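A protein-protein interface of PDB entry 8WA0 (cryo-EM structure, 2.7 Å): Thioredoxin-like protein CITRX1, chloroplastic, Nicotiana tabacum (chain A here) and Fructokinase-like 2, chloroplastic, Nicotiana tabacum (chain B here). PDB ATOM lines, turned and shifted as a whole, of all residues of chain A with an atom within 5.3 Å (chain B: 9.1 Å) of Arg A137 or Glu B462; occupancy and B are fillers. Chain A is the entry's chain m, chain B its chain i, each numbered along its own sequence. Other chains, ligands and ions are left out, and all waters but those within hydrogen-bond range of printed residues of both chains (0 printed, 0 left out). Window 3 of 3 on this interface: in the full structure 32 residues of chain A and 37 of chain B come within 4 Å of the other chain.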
ATOM      1  N   TYR A 133     -11.908 -20.383   5.805  1.00  0.00           N
ATOM      2  CA  TYR A 133     -12.367 -20.501   4.442  1.00  0.00           C
ATOM      3  C   TYR A 133     -11.372 -21.103   3.506  1.00  0.00           C
ATOM      4  O   TYR A 133     -11.717 -21.948   2.695  1.00  0.00           O
ATOM      5  CB  TYR A 133     -12.751 -19.134   3.931  1.00  0.00           C
ATOM      6  N   GLU A 134     -10.127 -20.681   3.602  1.00  0.00           N
ATOM      7  CA  GLU A 134      -9.079 -21.206   2.763  1.00  0.00           C
ATOM      8  C   GLU A 134      -8.757 -22.655   3.011  1.00  0.00           C
ATOM      9  O   GLU A 134      -8.521 -23.382   2.062  1.00  0.00           O
ATOM     10  CB  GLU A 134      -7.847 -20.355   2.905  1.00  0.00           C
ATOM     11  CG  GLU A 134      -8.003 -18.981   2.278  1.00  0.00           C
ATOM     12  CD  GLU A 134      -6.865 -18.046   2.629  1.00  0.00           C
ATOM     13  OE1 GLU A 134      -5.947 -18.474   3.359  1.00  0.00           O
ATOM     14  OE2 GLU A 134      -6.891 -16.882   2.177  1.00  0.00           O
ATOM     15  N   PHE A 135      -8.740 -23.108   4.247  1.00  0.00           N
ATOM     16  CA  PHE A 135      -8.377 -24.478   4.455  1.00  0.00           C
ATOM     17  C   PHE A 135      -9.396 -25.297   3.764  1.00  0.00           C
ATOM     18  O   PHE A 135      -9.100 -26.304   3.151  1.00  0.00           O
ATOM     19  CB  PHE A 135      -8.378 -24.827   5.915  1.00  0.00           C
ATOM     20  CG  PHE A 135      -7.999 -26.246   6.205  1.00  0.00           C
ATOM     21  CD1 PHE A 135      -6.709 -26.689   5.980  1.00  0.00           C
ATOM     22  CD2 PHE A 135      -8.922 -27.130   6.729  1.00  0.00           C
ATOM     23  CE1 PHE A 135      -6.354 -27.994   6.256  1.00  0.00           C
ATOM     24  CE2 PHE A 135      -8.574 -28.434   7.008  1.00  0.00           C
ATOM     25  CZ  PHE A 135      -7.290 -28.868   6.772  1.00  0.00           C
ATOM     26  N   ALA A 136     -10.632 -24.886   3.882  1.00  0.00           N
ATOM     27  CA  ALA A 136     -11.683 -25.639   3.285  1.00  0.00           C
ATOM     28  C   ALA A 136     -11.598 -25.657   1.782  1.00  0.00           C
ATOM     29  O   ALA A 136     -11.832 -26.697   1.177  1.00  0.00           O
ATOM     30  CB  ALA A 136     -13.017 -25.138   3.761  1.00  0.00           C
ATOM     31  N   ARG A 137     -11.263 -24.547   1.146  1.00  0.00           N
ATOM     32  CA  ARG A 137     -11.279 -24.576  -0.295  1.00  0.00           C
ATOM     33  C   ARG A 137     -10.262 -25.556  -0.781  1.00  0.00           C
ATOM     34  O   ARG A 137     -10.499 -26.259  -1.744  1.00  0.00           O
ATOM     35  CB  ARG A 137     -11.222 -23.205  -0.953  1.00  0.00           C
ATOM     36  CG  ARG A 137     -10.066 -22.316  -0.558  1.00  0.00           C
ATOM     37  CD  ARG A 137     -10.393 -20.870  -0.881  1.00  0.00           C
ATOM     38  NE  ARG A 137     -11.742 -20.524  -0.440  1.00  0.00           N
ATOM     39  CZ  ARG A 137     -12.259 -19.302  -0.501  1.00  0.00           C
ATOM     40  NH1 ARG A 137     -11.538 -18.299  -0.979  1.00  0.00           N
ATOM     41  NH2 ARG A 137     -13.495 -19.081  -0.078  1.00  0.00           N
ATOM     42  N   ASP A 138      -9.131 -25.628  -0.110  1.00  0.00           N
ATOM     43  CA  ASP A 138      -8.124 -26.601  -0.462  1.00  0.00           C
ATOM     44  C   ASP A 138      -8.505 -28.063  -0.289  1.00  0.00           C
ATOM     45  O   ASP A 138      -8.107 -28.898  -1.082  1.00  0.00           O
ATOM     46  CB  ASP A 138      -6.736 -26.256   0.081  1.00  0.00           C
ATOM     47  CG  ASP A 138      -6.582 -26.478   1.574  1.00  0.00           C
ATOM     48  OD1 ASP A 138      -6.795 -27.604   2.067  1.00  0.00           O
ATOM     49  OD2 ASP A 138      -6.182 -25.516   2.259  1.00  0.00           O
ATOM     50  N   MET A 139      -9.268 -28.409   0.712  1.00  0.00           N
ATOM     51  CA  MET A 139      -9.589 -29.789   0.880  1.00  0.00           C
ATOM     52  C   MET A 139     -10.853 -30.062   0.101  1.00  0.00           C
ATOM     53  O   MET A 139     -11.510 -31.063   0.313  1.00  0.00           O
ATOM     54  CB  MET A 139      -9.668 -30.156   2.340  1.00  0.00           C
ATOM     55  CG  MET A 139      -9.545 -31.629   2.649  1.00  0.00           C
ATOM     56  SD  MET A 139      -8.871 -31.854   4.298  1.00  0.00           S
ATOM     57  CE  MET A 139      -7.195 -31.285   4.029  1.00  0.00           C
ATOM     58  N   GLN A 140     -11.210 -29.169  -0.792  1.00  0.00           N
ATOM     59  CA  GLN A 140     -12.378 -29.343  -1.651  1.00  0.00           C
ATOM     60  C   GLN A 140     -13.782 -29.506  -1.089  1.00  0.00           C
ATOM     61  O   GLN A 140     -14.522 -30.364  -1.553  1.00  0.00           O
ATOM     62  CB  GLN A 140     -12.117 -30.372  -2.739  1.00  0.00           C
ATOM     63  CG  GLN A 140     -10.985 -30.023  -3.682  1.00  0.00           C
ATOM     64  CD  GLN A 140     -11.165 -28.668  -4.334  1.00  0.00           C
ATOM     65  OE1 GLN A 140     -12.272 -28.286  -4.710  1.00  0.00           O
ATOM     66  NE2 GLN A 140     -10.066 -27.937  -4.484  1.00  0.00           N
ATOM     67  N   VAL A 141     -14.164 -28.704  -0.102  1.00  0.00           N
ATOM     68  CA  VAL A 141     -15.527 -28.732   0.384  1.00  0.00           C
ATOM     69  C   VAL A 141     -16.405 -28.222  -0.713  1.00  0.00           C
ATOM     70  O   VAL A 141     -16.093 -27.247  -1.367  1.00  0.00           O
ATOM     71  CB  VAL A 141     -15.667 -27.826   1.576  1.00  0.00           C
ATOM     72  CG1 VAL A 141     -15.153 -26.433   1.298  1.00  0.00           C
ATOM     73  CG2 VAL A 141     -17.094 -27.794   2.087  1.00  0.00           C
ATOM     74  N   ARG B 295     -25.045 -17.200   3.208  1.00  0.00           N
ATOM     75  CA  ARG B 295     -24.581 -15.851   3.268  1.00  0.00           C
ATOM     76  C   ARG B 295     -25.407 -15.029   4.217  1.00  0.00           C
ATOM     77  O   ARG B 295     -26.550 -15.365   4.479  1.00  0.00           O
ATOM     78  CB  ARG B 295     -24.658 -15.277   1.875  1.00  0.00           C
ATOM     79  CG  ARG B 295     -23.780 -15.979   0.886  1.00  0.00           C
ATOM     80  CD  ARG B 295     -22.330 -15.735   1.221  1.00  0.00           C
ATOM     81  NE  ARG B 295     -22.025 -14.319   1.156  1.00  0.00           N
ATOM     82  CZ  ARG B 295     -20.802 -13.833   1.255  1.00  0.00           C
ATOM     83  NH1 ARG B 295     -19.783 -14.655   1.421  1.00  0.00           N
ATOM     84  NH2 ARG B 295     -20.601 -12.529   1.185  1.00  0.00           N
ATOM     85  N   GLY B 389      -0.261 -28.952   2.143  1.00  0.00           N
ATOM     86  CA  GLY B 389      -1.289 -27.927   2.152  1.00  0.00           C
ATOM     87  C   GLY B 389      -2.595 -28.670   2.008  1.00  0.00           C
ATOM     88  O   GLY B 389      -3.649 -28.065   1.850  1.00  0.00           O
ATOM     89  N   GLY B 390      -2.529 -29.993   2.041  1.00  0.00           N
ATOM     90  CA  GLY B 390      -3.732 -30.787   1.973  1.00  0.00           C
ATOM     91  C   GLY B 390      -4.589 -30.533   0.751  1.00  0.00           C
ATOM     92  O   GLY B 390      -5.810 -30.543   0.853  1.00  0.00           O
ATOM     93  N   LEU B 391      -3.986 -30.322  -0.410  1.00  0.00           N
ATOM     94  CA  LEU B 391      -4.810 -30.024  -1.553  1.00  0.00           C
ATOM     95  C   LEU B 391      -5.217 -31.359  -2.114  1.00  0.00           C
ATOM     96  O   LEU B 391      -4.441 -32.011  -2.795  1.00  0.00           O
ATOM     97  CB  LEU B 391      -4.030 -29.214  -2.575  1.00  0.00           C
ATOM     98  CG  LEU B 391      -4.734 -28.832  -3.879  1.00  0.00           C
ATOM     99  CD1 LEU B 391      -5.952 -27.963  -3.614  1.00  0.00           C
ATOM    100  CD2 LEU B 391      -3.765 -28.123  -4.810  1.00  0.00           C
ATOM    101  N   ARG B 392      -6.441 -31.776  -1.828  1.00  0.00           N
ATOM    102  CA  ARG B 392      -6.901 -33.082  -2.265  1.00  0.00           C
ATOM    103  C   ARG B 392      -7.189 -33.153  -3.741  1.00  0.00           C
ATOM    104  O   ARG B 392      -7.481 -32.140  -4.366  1.00  0.00           O
ATOM    105  CB  ARG B 392      -8.147 -33.472  -1.497  1.00  0.00           C
ATOM    106  CG  ARG B 392      -7.943 -33.665  -0.008  1.00  0.00           C
ATOM    107  CD  ARG B 392      -7.882 -35.140   0.336  1.00  0.00           C
ATOM    108  NE  ARG B 392      -8.128 -35.384   1.752  1.00  0.00           N
ATOM    109  CZ  ARG B 392      -7.178 -35.447   2.678  1.00  0.00           C
ATOM    110  NH1 ARG B 392      -5.904 -35.286   2.344  1.00  0.00           N
ATOM    111  NH2 ARG B 392      -7.502 -35.672   3.942  1.00  0.00           N
ATOM    112  N   LEU B 456     -24.846 -20.637  -6.272  1.00  0.00           N
ATOM    113  CA  LEU B 456     -23.401 -20.843  -6.219  1.00  0.00           C
ATOM    114  C   LEU B 456     -22.854 -21.600  -5.089  1.00  0.00           C
ATOM    115  O   LEU B 456     -23.116 -21.293  -3.943  1.00  0.00           O
ATOM    116  CB  LEU B 456     -22.647 -19.535  -6.360  1.00  0.00           C
ATOM    117  CG  LEU B 456     -22.630 -18.817  -7.696  1.00  0.00           C
ATOM    118  CD1 LEU B 456     -21.734 -17.600  -7.572  1.00  0.00           C
ATOM    119  CD2 LEU B 456     -22.119 -19.745  -8.782  1.00  0.00           C
ATOM    120  N   PRO B 457     -22.080 -22.679  -5.397  1.00  0.00           N
ATOM    121  CA  PRO B 457     -21.639 -23.442  -4.237  1.00  0.00           C
ATOM    122  C   PRO B 457     -20.472 -22.821  -3.513  1.00  0.00           C
ATOM    123  O   PRO B 457     -19.990 -21.786  -3.932  1.00  0.00           O
ATOM    124  CB  PRO B 457     -21.229 -24.781  -4.838  1.00  0.00           C
ATOM    125  CG  PRO B 457     -21.872 -24.835  -6.176  1.00  0.00           C
ATOM    126  CD  PRO B 457     -21.760 -23.426  -6.634  1.00  0.00           C
ATOM    127  N   PHE B 458     -19.983 -23.472  -2.471  1.00  0.00           N
ATOM    128  CA  PHE B 458     -18.920 -22.909  -1.652  1.00  0.00           C
ATOM    129  C   PHE B 458     -17.618 -22.627  -2.382  1.00  0.00           C
ATOM    130  O   PHE B 458     -17.009 -21.589  -2.162  1.00  0.00           O
ATOM    131  CB  PHE B 458     -18.666 -23.855  -0.478  1.00  0.00           C
ATOM    132  CG  PHE B 458     -17.910 -23.246   0.666  1.00  0.00           C
ATOM    133  CD1 PHE B 458     -16.526 -23.252   0.688  1.00  0.00           C
ATOM    134  CD2 PHE B 458     -18.586 -22.703   1.741  1.00  0.00           C
ATOM    135  CE1 PHE B 458     -15.830 -22.705   1.747  1.00  0.00           C
ATOM    136  CE2 PHE B 458     -17.898 -22.157   2.806  1.00  0.00           C
ATOM    137  CZ  PHE B 458     -16.517 -22.157   2.810  1.00  0.00           C
ATOM    138  N   PRO B 459     -17.176 -23.533  -3.260  1.00  0.00           N
ATOM    139  CA  PRO B 459     -15.905 -23.190  -3.887  1.00  0.00           C
ATOM    140  C   PRO B 459     -15.875 -21.910  -4.671  1.00  0.00           C
ATOM    141  O   PRO B 459     -14.891 -21.193  -4.575  1.00  0.00           O
ATOM    142  CB  PRO B 459     -15.707 -24.328  -4.871  1.00  0.00           C
ATOM    143  CG  PRO B 459     -16.357 -25.489  -4.227  1.00  0.00           C
ATOM    144  CD  PRO B 459     -17.576 -24.916  -3.581  1.00  0.00           C
ATOM    145  N   LEU B 460     -16.915 -21.599  -5.420  1.00  0.00           N
ATOM    146  CA  LEU B 460     -16.847 -20.455  -6.302  1.00  0.00           C
ATOM    147  C   LEU B 460     -16.975 -19.053  -5.762  1.00  0.00           C
ATOM    148  O   LEU B 460     -17.138 -18.128  -6.532  1.00  0.00           O
ATOM    149  CB  LEU B 460     -17.775 -20.606  -7.493  1.00  0.00           C
ATOM    150  CG  LEU B 460     -17.654 -21.758  -8.481  1.00  0.00           C
ATOM    151  CD1 LEU B 460     -18.452 -22.958  -8.004  1.00  0.00           C
ATOM    152  CD2 LEU B 460     -18.207 -21.279  -9.807  1.00  0.00           C
ATOM    153  N   TRP B 461     -16.925 -18.877  -4.458  1.00  0.00           N
ATOM    154  CA  TRP B 461     -17.062 -17.569  -3.862  1.00  0.00           C
ATOM    155  C   TRP B 461     -15.782 -16.820  -3.658  1.00  0.00           C
ATOM    156  O   TRP B 461     -15.790 -15.758  -3.060  1.00  0.00           O
ATOM    157  CB  TRP B 461     -17.799 -17.636  -2.534  1.00  0.00           C
ATOM    158  CG  TRP B 461     -19.261 -17.941  -2.646  1.00  0.00           C
ATOM    159  CD1 TRP B 461     -19.818 -19.160  -2.797  1.00  0.00           C
ATOM    160  CD2 TRP B 461     -20.347 -17.011  -2.599  1.00  0.00           C
ATOM    161  NE1 TRP B 461     -21.178 -19.060  -2.864  1.00  0.00           N
ATOM    162  CE2 TRP B 461     -21.527 -17.744  -2.746  1.00  0.00           C
ATOM    163  CE3 TRP B 461     -20.433 -15.633  -2.451  1.00  0.00           C
ATOM    164  CZ2 TRP B 461     -22.775 -17.147  -2.751  1.00  0.00           C
ATOM    165  CZ3 TRP B 461     -21.664 -15.044  -2.464  1.00  0.00           C
ATOM    166  CH2 TRP B 461     -22.819 -15.793  -2.613  1.00  0.00           C
ATOM    167  N   GLU B 462     -14.671 -17.360  -4.121  1.00  0.00           N
ATOM    168  CA  GLU B 462     -13.404 -16.720  -3.912  1.00  0.00           C
ATOM    169  C   GLU B 462     -13.326 -15.367  -4.544  1.00  0.00           C
ATOM    170  O   GLU B 462     -12.898 -14.421  -3.906  1.00  0.00           O
ATOM    171  CB  GLU B 462     -12.314 -17.575  -4.493  1.00  0.00           C
ATOM    172  N   SER B 463     -13.760 -15.241  -5.779  1.00  0.00           N
ATOM    173  CA  SER B 463     -13.766 -13.958  -6.416  1.00  0.00           C
ATOM    174  C   SER B 463     -14.753 -13.873  -7.504  1.00  0.00           C
ATOM    175  O   SER B 463     -15.017 -14.843  -8.177  1.00  0.00           O
ATOM    176  CB  SER B 463     -12.388 -13.626  -6.974  1.00  0.00           C
ATOM    177  OG  SER B 463     -11.888 -14.691  -7.759  1.00  0.00           O
ATOM    178  N   GLY B 464     -15.263 -12.687  -7.723  1.00  0.00           N
ATOM    179  CA  GLY B 464     -16.281 -12.484  -8.715  1.00  0.00           C
ATOM    180  C   GLY B 464     -15.932 -12.727 -10.130  1.00  0.00           C
ATOM    181  O   GLY B 464     -16.737 -13.238 -10.893  1.00  0.00           O
ATOM    182  N   ASP B 465     -14.747 -12.335 -10.514  1.00  0.00           N
ATOM    183  CA  ASP B 465     -14.388 -12.475 -11.874  1.00  0.00           C
ATOM    184  C   ASP B 465     -14.376 -13.933 -12.218  1.00  0.00           C
ATOM    185  O   ASP B 465     -14.848 -14.330 -13.275  1.00  0.00           O
ATOM    186  CB  ASP B 465     -13.017 -11.873 -12.090  1.00  0.00           C
ATOM    187  CG  ASP B 465     -12.636 -11.804 -13.557  1.00  0.00           C
ATOM    188  OD1 ASP B 465     -13.542 -11.669 -14.407  1.00  0.00           O
ATOM    189  OD2 ASP B 465     -11.426 -11.871 -13.861  1.00  0.00           O
ATOM    190  N   LYS B 466     -13.868 -14.751 -11.325  1.00  0.00           N
ATOM    191  CA  LYS B 466     -13.774 -16.152 -11.621  1.00  0.00           C
ATOM    192  C   LYS B 466     -15.135 -16.739 -11.830  1.00  0.00           C
ATOM    193  O   LYS B 466     -15.333 -17.552 -12.721  1.00  0.00           O
ATOM    194  CB  LYS B 466     -13.052 -16.869 -10.501  1.00  0.00           C
ATOM    195  CG  LYS B 466     -11.580 -16.527 -10.412  1.00  0.00           C
ATOM    196  CD  LYS B 466     -10.876 -16.783 -11.734  1.00  0.00           C
ATOM    197  CE  LYS B 466      -9.410 -16.390 -11.653  1.00  0.00           C
ATOM    198  NZ  LYS B 466      -8.710 -17.120 -10.561  1.00  0.00           N
ATOM    199  N   ALA B 467     -16.092 -16.340 -11.018  1.00  0.00           N
ATOM    200  CA  ALA B 467     -17.443 -16.826 -11.149  1.00  0.00           C
ATOM    201  C   ALA B 467     -18.108 -16.449 -12.415  1.00  0.00           C
ATOM    202  O   ALA B 467     -18.745 -17.285 -13.030  1.00  0.00           O
ATOM    203  CB  ALA B 467     -18.270 -16.323 -10.006  1.00  0.00           C
ATOM    204  N   PHE B 490     -22.571  -9.933  -5.909  1.00  0.00           N
ATOM    205  CA  PHE B 490     -21.253 -10.519  -6.048  1.00  0.00           C
ATOM    206  C   PHE B 490     -20.827 -10.586  -7.495  1.00  0.00           C
ATOM    207  O   PHE B 490     -19.704 -10.230  -7.824  1.00  0.00           O
ATOM    208  CB  PHE B 490     -21.293 -11.917  -5.442  1.00  0.00           C
ATOM    209  CG  PHE B 490     -19.999 -12.665  -5.496  1.00  0.00           C
ATOM    210  CD1 PHE B 490     -18.913 -12.259  -4.747  1.00  0.00           C
ATOM    211  CD2 PHE B 490     -19.893 -13.819  -6.249  1.00  0.00           C
ATOM    212  CE1 PHE B 490     -17.731 -12.968  -4.781  1.00  0.00           C
ATOM    213  CE2 PHE B 490     -18.714 -14.533  -6.287  1.00  0.00           C
ATOM    214  CZ  PHE B 490     -17.632 -14.108  -5.549  1.00  0.00           C
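N of Arg B392 lies within hydrogen-bond range of O of Asp A138, at 3.4 Å. The backbone carbonyl oxygen (O) of Gly B389 lies close to the side-chain carboxylate (OD1) of Asp A138, 3.2 Å away. OD1 of Asp A138 sits close to O of Gly B390, at 3.3 Å.
NE of Arg A137 sits at hydrogen-bond distance from O of Tyr A133, 3.4 Å away. The backbone NH (N) of Val A141 is in hydrogen-bond range of the backbone carbonyl oxygen (O) of Ala A136 (3.3 Å). The backbone carbonyl oxygen of Arg A137 is in hydrogen-bond range of the side-chain amide nitrogen of Gln A140 (3.2 Å).
Among the printed residues, merely in contact across the chains: Val A141 with Pro B459 (3.4 Å), Asp A138 with Leu B391 (3.5 Å), Val A141 with Phe B458 (3.5 Å), Met A139 with Gly B390 (3.5 Å), Arg A137 with Glu B462 (3.7 Å) and Met A139 with Arg B392 (3.7 Å).
Of the printed residues of chain B, Arg A137 touches Glu B462 (3.7 Å). Printed residues of chain A within 4 Å of Gly B389: Asp A138. Of the printed residues of chain A, Gly B390 touches Asp A138 (3.3 Å) and Met A139 (3.5 Å). Of the printed residues of chain A, Pro B459 touches Val A141. Printed residues of chain A within 4 Å of Glu B462: Arg A137. The nearest printed residue of chain A that does not touch Glu B462 is Glu A134 (8.1 Å). The nearest printed residue of chain A that does not touch Arg B392 is Gln A140 (4.2 Å).
Of the 18 printed residues of chain B, 7 touch a printed residue of chain A. Hydrophobic or aromatic side chains of chain B within 4 Å of the printed part of chain A: Leu B391, Phe B458 and Pro B459. Among the printed residues, no Asp or Glu carboxylate lies within 4 Å of a Lys or Arg side-chain nitrogen of the other chain.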
